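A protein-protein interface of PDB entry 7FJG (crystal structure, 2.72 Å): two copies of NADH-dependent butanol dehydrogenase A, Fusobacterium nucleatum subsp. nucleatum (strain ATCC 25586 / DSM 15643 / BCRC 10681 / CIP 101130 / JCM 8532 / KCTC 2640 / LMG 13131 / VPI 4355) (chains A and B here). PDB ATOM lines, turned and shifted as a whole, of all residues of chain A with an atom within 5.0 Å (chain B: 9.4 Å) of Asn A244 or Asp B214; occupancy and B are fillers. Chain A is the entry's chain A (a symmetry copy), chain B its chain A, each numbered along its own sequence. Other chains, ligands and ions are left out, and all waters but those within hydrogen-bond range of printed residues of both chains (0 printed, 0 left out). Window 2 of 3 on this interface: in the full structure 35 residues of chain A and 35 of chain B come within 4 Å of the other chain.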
ATOM      1  N   TYR A 232     -19.814 -25.158  32.600  1.00  0.00           N
ATOM      2  CA  TYR A 232     -21.084 -25.595  33.194  1.00  0.00           C
ATOM      3  C   TYR A 232     -20.968 -26.833  34.083  1.00  0.00           C
ATOM      4  O   TYR A 232     -21.624 -26.883  35.135  1.00  0.00           O
ATOM      5  CB  TYR A 232     -22.153 -25.805  32.094  1.00  0.00           C
ATOM      6  CG  TYR A 232     -22.760 -24.457  31.681  1.00  0.00           C
ATOM      7  CD1 TYR A 232     -22.132 -23.633  30.745  1.00  0.00           C
ATOM      8  CD2 TYR A 232     -23.909 -23.991  32.270  1.00  0.00           C
ATOM      9  CE1 TYR A 232     -22.642 -22.396  30.406  1.00  0.00           C
ATOM     10  CE2 TYR A 232     -24.451 -22.741  31.925  1.00  0.00           C
ATOM     11  CZ  TYR A 232     -23.809 -21.942  31.012  1.00  0.00           C
ATOM     12  OH  TYR A 232     -24.350 -20.699  30.717  1.00  0.00           O
ATOM     13  N   ASN A 242     -30.831 -28.212  37.890  1.00  0.00           N
ATOM     14  CA  ASN A 242     -30.978 -26.996  37.096  1.00  0.00           C
ATOM     15  C   ASN A 242     -31.097 -27.331  35.608  1.00  0.00           C
ATOM     16  O   ASN A 242     -30.124 -27.750  34.974  1.00  0.00           O
ATOM     17  CB  ASN A 242     -29.805 -26.072  37.411  1.00  0.00           C
ATOM     18  CG  ASN A 242     -29.834 -24.839  36.586  1.00  0.00           C
ATOM     19  OD1 ASN A 242     -30.129 -24.883  35.379  1.00  0.00           O
ATOM     20  ND2 ASN A 242     -29.514 -23.719  37.212  1.00  0.00           N
ATOM     21  N   TYR A 243     -32.283 -27.114  35.031  1.00  0.00           N
ATOM     22  CA  TYR A 243     -32.547 -27.635  33.686  1.00  0.00           C
ATOM     23  C   TYR A 243     -31.600 -27.048  32.641  1.00  0.00           C
ATOM     24  O   TYR A 243     -31.168 -27.758  31.732  1.00  0.00           O
ATOM     25  CB  TYR A 243     -33.985 -27.350  33.275  1.00  0.00           C
ATOM     26  CG  TYR A 243     -34.285 -27.899  31.927  1.00  0.00           C
ATOM     27  CD1 TYR A 243     -34.566 -29.244  31.770  1.00  0.00           C
ATOM     28  CD2 TYR A 243     -34.211 -27.096  30.781  1.00  0.00           C
ATOM     29  CE1 TYR A 243     -34.794 -29.775  30.528  1.00  0.00           C
ATOM     30  CE2 TYR A 243     -34.463 -27.623  29.536  1.00  0.00           C
ATOM     31  CZ  TYR A 243     -34.753 -28.966  29.420  1.00  0.00           C
ATOM     32  OH  TYR A 243     -34.998 -29.524  28.198  1.00  0.00           O
ATOM     33  N   ASN A 244     -31.322 -25.741  32.725  1.00  0.00           N
ATOM     34  CA  ASN A 244     -30.388 -25.071  31.821  1.00  0.00           C
ATOM     35  C   ASN A 244     -29.021 -25.734  31.857  1.00  0.00           C
ATOM     36  O   ASN A 244     -28.500 -26.167  30.826  1.00  0.00           O
ATOM     37  CB  ASN A 244     -30.271 -23.586  32.207  1.00  0.00           C
ATOM     38  CG  ASN A 244     -29.110 -22.865  31.528  1.00  0.00           C
ATOM     39  OD1 ASN A 244     -28.856 -23.020  30.336  1.00  0.00           O
ATOM     40  ND2 ASN A 244     -28.414 -22.036  32.304  1.00  0.00           N
ATOM     41  N   TYR A 245     -28.414 -25.784  33.041  1.00  0.00           N
ATOM     42  CA  TYR A 245     -27.116 -26.424  33.200  1.00  0.00           C
ATOM     43  C   TYR A 245     -27.103 -27.851  32.634  1.00  0.00           C
ATOM     44  O   TYR A 245     -26.124 -28.281  31.987  1.00  0.00           O
ATOM     45  CB  TYR A 245     -26.773 -26.443  34.681  1.00  0.00           C
ATOM     46  CG  TYR A 245     -26.601 -25.085  35.350  1.00  0.00           C
ATOM     47  CD1 TYR A 245     -26.540 -23.924  34.624  1.00  0.00           C
ATOM     48  CD2 TYR A 245     -26.450 -24.995  36.724  1.00  0.00           C
ATOM     49  CE1 TYR A 245     -26.330 -22.721  35.236  1.00  0.00           C
ATOM     50  CE2 TYR A 245     -26.237 -23.791  37.343  1.00  0.00           C
ATOM     51  CZ  TYR A 245     -26.183 -22.652  36.601  1.00  0.00           C
ATOM     52  OH  TYR A 245     -25.997 -21.418  37.220  1.00  0.00           O
ATOM     53  N   CYS A 246     -28.175 -28.609  32.883  1.00  0.00           N
ATOM     54  CA  CYS A 246     -28.239 -29.970  32.363  1.00  0.00           C
ATOM     55  C   CYS A 246     -28.379 -29.989  30.849  1.00  0.00           C
ATOM     56  O   CYS A 246     -27.891 -30.920  30.200  1.00  0.00           O
ATOM     57  CB  CYS A 246     -29.413 -30.725  32.979  1.00  0.00           C
ATOM     58  SG  CYS A 246     -29.062 -31.315  34.611  1.00  0.00           S
ATOM     59  N   SER A 247     -29.039 -28.976  30.280  1.00  0.00           N
ATOM     60  CA  SER A 247     -29.246 -28.919  28.834  1.00  0.00           C
ATOM     61  C   SER A 247     -27.951 -28.618  28.097  1.00  0.00           C
ATOM     62  O   SER A 247     -27.681 -29.189  27.034  1.00  0.00           O
ATOM     63  CB  SER A 247     -30.299 -27.855  28.475  1.00  0.00           C
ATOM     64  OG  SER A 247     -31.522 -28.104  29.144  1.00  0.00           O
ATOM     65  N   GLN A 248     -27.148 -27.701  28.612  1.00  0.00           N
ATOM     66  CA  GLN A 248     -25.860 -27.462  27.965  1.00  0.00           C
ATOM     67  C   GLN A 248     -24.999 -28.726  28.005  1.00  0.00           C
ATOM     68  O   GLN A 248     -24.390 -29.112  26.997  1.00  0.00           O
ATOM     69  CB  GLN A 248     -25.139 -26.295  28.637  1.00  0.00           C
ATOM     70  CG  GLN A 248     -26.011 -25.089  28.820  1.00  0.00           C
ATOM     71  CD  GLN A 248     -26.690 -24.764  27.570  1.00  0.00           C
ATOM     72  OE1 GLN A 248     -26.042 -24.446  26.567  1.00  0.00           O
ATOM     73  NE2 GLN A 248     -28.017 -24.895  27.573  1.00  0.00           N
ATOM     74  N   ASP B   2     -38.206 -24.259  24.988  1.00  0.00           N
ATOM     75  CA  ASP B   2     -37.137 -24.253  23.981  1.00  0.00           C
ATOM     76  C   ASP B   2     -36.609 -25.639  23.636  1.00  0.00           C
ATOM     77  O   ASP B   2     -35.401 -25.862  23.699  1.00  0.00           O
ATOM     78  CB  ASP B   2     -35.955 -23.400  24.465  1.00  0.00           C
ATOM     79  CG  ASP B   2     -35.463 -23.820  25.857  1.00  0.00           C
ATOM     80  OD1 ASP B   2     -36.153 -24.668  26.465  1.00  0.00           O
ATOM     81  OD2 ASP B   2     -34.423 -23.303  26.356  1.00  0.00           O
ATOM     82  N   ASN B   3     -37.516 -26.560  23.301  1.00  0.00           N
ATOM     83  CA  ASN B   3     -37.189 -27.887  22.802  1.00  0.00           C
ATOM     84  C   ASN B   3     -37.005 -27.849  21.280  1.00  0.00           C
ATOM     85  O   ASN B   3     -37.291 -26.849  20.609  1.00  0.00           O
ATOM     86  CB  ASN B   3     -38.292 -28.875  23.166  1.00  0.00           C
ATOM     87  CG  ASN B   3     -38.480 -29.069  24.687  1.00  0.00           C
ATOM     88  OD1 ASN B   3     -37.774 -28.485  25.543  1.00  0.00           O
ATOM     89  ND2 ASN B   3     -39.434 -29.932  25.020  1.00  0.00           N
ATOM     90  N   PHE B   4     -36.491 -28.945  20.726  1.00  0.00           N
ATOM     91  CA  PHE B   4     -36.198 -28.945  19.297  1.00  0.00           C
ATOM     92  C   PHE B   4     -35.954 -30.376  18.830  1.00  0.00           C
ATOM     93  O   PHE B   4     -35.600 -31.258  19.626  1.00  0.00           O
ATOM     94  CB  PHE B   4     -34.998 -28.010  18.954  1.00  0.00           C
ATOM     95  CG  PHE B   4     -33.669 -28.531  19.389  1.00  0.00           C
ATOM     96  CD1 PHE B   4     -32.931 -29.363  18.572  1.00  0.00           C
ATOM     97  CD2 PHE B   4     -33.166 -28.210  20.642  1.00  0.00           C
ATOM     98  CE1 PHE B   4     -31.699 -29.881  18.991  1.00  0.00           C
ATOM     99  CE2 PHE B   4     -31.945 -28.721  21.074  1.00  0.00           C
ATOM    100  CZ  PHE B   4     -31.204 -29.562  20.241  1.00  0.00           C
ATOM    101  N   THR B 210     -31.249 -13.265  18.920  1.00  0.00           N
ATOM    102  CA  THR B 210     -32.455 -13.964  19.298  1.00  0.00           C
ATOM    103  C   THR B 210     -32.844 -13.548  20.702  1.00  0.00           C
ATOM    104  O   THR B 210     -31.981 -13.263  21.540  1.00  0.00           O
ATOM    105  CB  THR B 210     -32.290 -15.493  19.263  1.00  0.00           C
ATOM    106  OG1 THR B 210     -33.592 -16.087  19.236  1.00  0.00           O
ATOM    107  CG2 THR B 210     -31.544 -16.012  20.485  1.00  0.00           C
ATOM    108  N   LYS B 211     -34.172 -13.545  20.942  1.00  0.00           N
ATOM    109  CA  LYS B 211     -34.751 -13.290  22.257  1.00  0.00           C
ATOM    110  C   LYS B 211     -34.746 -14.549  23.124  1.00  0.00           C
ATOM    111  O   LYS B 211     -35.073 -14.456  24.321  1.00  0.00           O
ATOM    112  CB  LYS B 211     -36.157 -12.682  22.075  1.00  0.00           C
ATOM    113  CG  LYS B 211     -36.085 -11.159  21.762  1.00  0.00           C
ATOM    114  CD  LYS B 211     -37.368 -10.563  21.128  1.00  0.00           C
ATOM    115  CE  LYS B 211     -38.508 -10.502  22.122  1.00  0.00           C
ATOM    116  NZ  LYS B 211     -39.865 -10.703  21.465  1.00  0.00           N
ATOM    117  N   SER B 212     -34.322 -15.696  22.567  1.00  0.00           N
ATOM    118  CA  SER B 212     -34.313 -16.946  23.316  1.00  0.00           C
ATOM    119  C   SER B 212     -33.239 -16.890  24.391  1.00  0.00           C
ATOM    120  O   SER B 212     -32.328 -16.059  24.352  1.00  0.00           O
ATOM    121  CB  SER B 212     -34.071 -18.165  22.404  1.00  0.00           C
ATOM    122  OG  SER B 212     -34.778 -18.140  21.158  1.00  0.00           O
ATOM    123  N   ILE B 213     -33.339 -17.805  25.352  1.00  0.00           N
ATOM    124  CA  ILE B 213     -32.436 -17.860  26.496  1.00  0.00           C
ATOM    125  C   ILE B 213     -31.982 -19.300  26.691  1.00  0.00           C
ATOM    126  O   ILE B 213     -32.538 -20.237  26.112  1.00  0.00           O
ATOM    127  CB  ILE B 213     -33.113 -17.353  27.787  1.00  0.00           C
ATOM    128  CG1 ILE B 213     -34.293 -18.277  28.111  1.00  0.00           C
ATOM    129  CG2 ILE B 213     -33.561 -15.918  27.634  1.00  0.00           C
ATOM    130  CD1 ILE B 213     -34.849 -18.087  29.466  1.00  0.00           C
ATOM    131  N   ASP B 214     -31.003 -19.480  27.577  1.00  0.00           N
ATOM    132  CA  ASP B 214     -30.523 -20.815  27.912  1.00  0.00           C
ATOM    133  C   ASP B 214     -29.898 -21.482  26.685  1.00  0.00           C
ATOM    134  O   ASP B 214     -30.183 -22.640  26.354  1.00  0.00           O
ATOM    135  CB  ASP B 214     -31.656 -21.674  28.489  1.00  0.00           C
ATOM    136  CG  ASP B 214     -32.057 -21.246  29.921  1.00  0.00           C
ATOM    137  OD1 ASP B 214     -31.466 -20.248  30.442  1.00  0.00           O
ATOM    138  OD2 ASP B 214     -32.943 -21.927  30.525  1.00  0.00           O
ATOM    139  N   THR B 215     -29.020 -20.746  26.007  1.00  0.00           N
ATOM    140  CA  THR B 215     -28.519 -21.186  24.707  1.00  0.00           C
ATOM    141  C   THR B 215     -26.997 -21.145  24.604  1.00  0.00           C
ATOM    142  O   THR B 215     -26.477 -20.932  23.505  1.00  0.00           O
ATOM    143  CB  THR B 215     -29.098 -20.319  23.593  1.00  0.00           C
ATOM    144  OG1 THR B 215     -29.094 -18.933  24.011  1.00  0.00           O
ATOM    145  CG2 THR B 215     -30.457 -20.728  23.288  1.00  0.00           C
ATOM    146  N   ALA B 216     -26.287 -21.373  25.724  1.00  0.00           N
ATOM    147  CA  ALA B 216     -24.863 -21.065  25.826  1.00  0.00           C
ATOM    148  C   ALA B 216     -24.040 -21.880  24.836  1.00  0.00           C
ATOM    149  O   ALA B 216     -23.305 -21.326  23.997  1.00  0.00           O
ATOM    150  CB  ALA B 216     -24.364 -21.341  27.243  1.00  0.00           C
ATOM    151  N   LEU B 217     -24.127 -23.208  24.953  1.00  0.00           N
ATOM    152  CA  LEU B 217     -23.452 -24.079  24.008  1.00  0.00           C
ATOM    153  C   LEU B 217     -23.686 -23.620  22.579  1.00  0.00           C
ATOM    154  O   LEU B 217     -22.732 -23.394  21.812  1.00  0.00           O
ATOM    155  CB  LEU B 217     -23.929 -25.508  24.162  1.00  0.00           C
ATOM    156  CG  LEU B 217     -23.357 -26.460  23.134  1.00  0.00           C
ATOM    157  CD1 LEU B 217     -21.879 -26.236  23.102  1.00  0.00           C
ATOM    158  CD2 LEU B 217     -23.679 -27.869  23.628  1.00  0.00           C
ATOM    159  N   SER B 218     -24.955 -23.496  22.193  1.00  0.00           N
ATOM    160  CA  SER B 218     -25.241 -23.083  20.827  1.00  0.00           C
ATOM    161  C   SER B 218     -24.648 -21.701  20.528  1.00  0.00           C
ATOM    162  O   SER B 218     -24.087 -21.470  19.443  1.00  0.00           O
ATOM    163  CB  SER B 218     -26.745 -23.130  20.604  1.00  0.00           C
ATOM    164  OG  SER B 218     -27.136 -22.206  19.613  1.00  0.00           O
ATOM    165  N   ASP B 219     -24.729 -20.774  21.479  1.00  0.00           N
ATOM    166  CA  ASP B 219     -24.057 -19.493  21.302  1.00  0.00           C
ATOM    167  C   ASP B 219     -22.601 -19.706  20.888  1.00  0.00           C
ATOM    168  O   ASP B 219     -22.086 -19.064  19.957  1.00  0.00           O
ATOM    169  CB  ASP B 219     -24.124 -18.704  22.608  1.00  0.00           C
ATOM    170  CG  ASP B 219     -25.476 -18.012  22.860  1.00  0.00           C
ATOM    171  OD1 ASP B 219     -26.469 -18.126  22.081  1.00  0.00           O
ATOM    172  OD2 ASP B 219     -25.509 -17.317  23.896  1.00  0.00           O
ATOM    173  N   CYS B 263     -29.976 -24.504  17.693  1.00  0.00           N
ATOM    174  CA  CYS B 263     -30.826 -25.618  18.134  1.00  0.00           C
ATOM    175  C   CYS B 263     -31.863 -25.126  19.125  1.00  0.00           C
ATOM    176  O   CYS B 263     -31.594 -25.069  20.329  1.00  0.00           O
ATOM    177  CB  CYS B 263     -30.017 -26.775  18.725  1.00  0.00           C
ATOM    178  SG  CYS B 263     -28.717 -26.458  20.039  1.00  0.00           S
ATOM    179  N   GLY B 264     -33.059 -24.831  18.615  1.00  0.00           N
ATOM    180  CA  GLY B 264     -34.081 -24.294  19.476  1.00  0.00           C
ATOM    181  C   GLY B 264     -33.817 -22.828  19.738  1.00  0.00           C
ATOM    182  O   GLY B 264     -33.749 -22.365  20.884  1.00  0.00           O
ATOM    183  N   ARG B 265     -33.661 -22.081  18.662  1.00  0.00           N
ATOM    184  CA  ARG B 265     -33.564 -20.642  18.797  1.00  0.00           C
ATOM    185  C   ARG B 265     -34.228 -19.979  17.609  1.00  0.00           C
ATOM    186  O   ARG B 265     -34.147 -20.485  16.472  1.00  0.00           O
ATOM    187  CB  ARG B 265     -32.123 -20.169  18.906  1.00  0.00           C
ATOM    188  CG  ARG B 265     -31.222 -20.647  17.829  1.00  0.00           C
ATOM    189  CD  ARG B 265     -29.848 -20.509  18.360  1.00  0.00           C
ATOM    190  NE  ARG B 265     -29.511 -19.107  18.540  1.00  0.00           N
ATOM    191  CZ  ARG B 265     -28.518 -18.678  19.308  1.00  0.00           C
ATOM    192  NH1 ARG B 265     -28.230 -17.385  19.403  1.00  0.00           N
ATOM    193  NH2 ARG B 265     -27.807 -19.545  19.998  1.00  0.00           N
ATOM    194  N   ILE B 308     -26.918  -9.377  24.603  1.00  0.00           N
ATOM    195  CA  ILE B 308     -26.573 -10.329  23.567  1.00  0.00           C
ATOM    196  C   ILE B 308     -25.786  -9.636  22.455  1.00  0.00           C
ATOM    197  O   ILE B 308     -25.069 -10.306  21.692  1.00  0.00           O
ATOM    198  CB  ILE B 308     -27.754 -11.131  22.991  1.00  0.00           C
ATOM    199  CG1 ILE B 308     -27.153 -12.475  22.496  1.00  0.00           C
ATOM    200  CG2 ILE B 308     -28.382 -10.391  21.859  1.00  0.00           C
ATOM    201  CD1 ILE B 308     -28.128 -13.657  22.184  1.00  0.00           C
ATOM    202  N   LYS B 311     -22.219  -9.584  24.031  1.00  0.00           N
ATOM    203  CA  LYS B 311     -21.653 -10.914  23.851  1.00  0.00           C
ATOM    204  C   LYS B 311     -21.162 -11.086  22.418  1.00  0.00           C
ATOM    205  O   LYS B 311     -19.973 -11.323  22.172  1.00  0.00           O
ATOM    206  CB  LYS B 311     -22.668 -11.979  24.199  1.00  0.00           C
ATOM    207  CG  LYS B 311     -22.045 -13.366  24.264  1.00  0.00           C
ATOM    208  CD  LYS B 311     -23.044 -14.363  24.851  1.00  0.00           C
ATOM    209  CE  LYS B 311     -22.448 -15.696  25.041  1.00  0.00           C
ATOM    210  NZ  LYS B 311     -23.488 -16.766  24.977  1.00  0.00           N
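Of the printed residues of chain B, Tyr A232 touches Ala B216.
Of the printed residues of chain B, Tyr A243 touches Asn B3.
Of the printed residues of chain A, Asn B3 touches Tyr A243 (3.98 Å).
Printed residues of chain A within 4 Å of Asp B214: Asn A244 (3.6 Å) and Gln A248 (3.4 Å).
Printed residues of chain A within 4 Å of Thr B215: Gln A248.
Printed residues of chain A within 4 Å of Ala B216: Tyr A232 (3.5 Å) and Gln A248 (3.2 Å).
The nearest printed residue of chain A that does not touch Asn B3 is Ser A247 (7.2 Å).
No position is printed for both chains.
The side-chain hydroxyl of Thr B215 sits at hydrogen-bond distance from the side-chain carboxylate of Asp B219, at 3.4 Å.
The backbone NH of Asn A244 sits at hydrogen-bond distance from the side-chain amide oxygen of Asn A242, at 3.0 Å.
The backbone carbonyl oxygen of Tyr A243 lies within hydrogen-bond range of the side-chain hydroxyl of Ser A247 (2.6 Å).
The side-chain amide oxygen of Asn A244 lies within hydrogen-bond range of the side-chain amide nitrogen of Gln A248.
Among the printed residues, pairs that only touch across the chains: Tyr A232 with Ala B216 (3.5 Å), Tyr A243 with Asn B3 (3.98 Å), Asn A244 with Asp B214 (3.6 Å) and Gln A248 with Thr B215 (3.96 Å).
O of Asp B214 sits at hydrogen-bond distance from NE2 of Gln A248 (3.4 Å).
OE1 of Gln A248 lies within hydrogen-bond range of N of Ala B216 (3.2 Å).
The backbone NH of Leu B217 is in hydrogen-bond range of the side-chain amide oxygen of Gln A248, at 2.8 Å.
Hydrophobic or aromatic side chains of chain B within 4 Å of the printed part of chain A: Ala B216 and Leu B217.
Of the 8 printed residues of chain A, 4 touch a printed residue of chain B.
Among the printed residues, 7 pairs touch across the chains.
Among the printed residues, no Asp or Glu carboxylate lies within 4 Å of a Lys or Arg side-chain nitrogen of the other chain.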
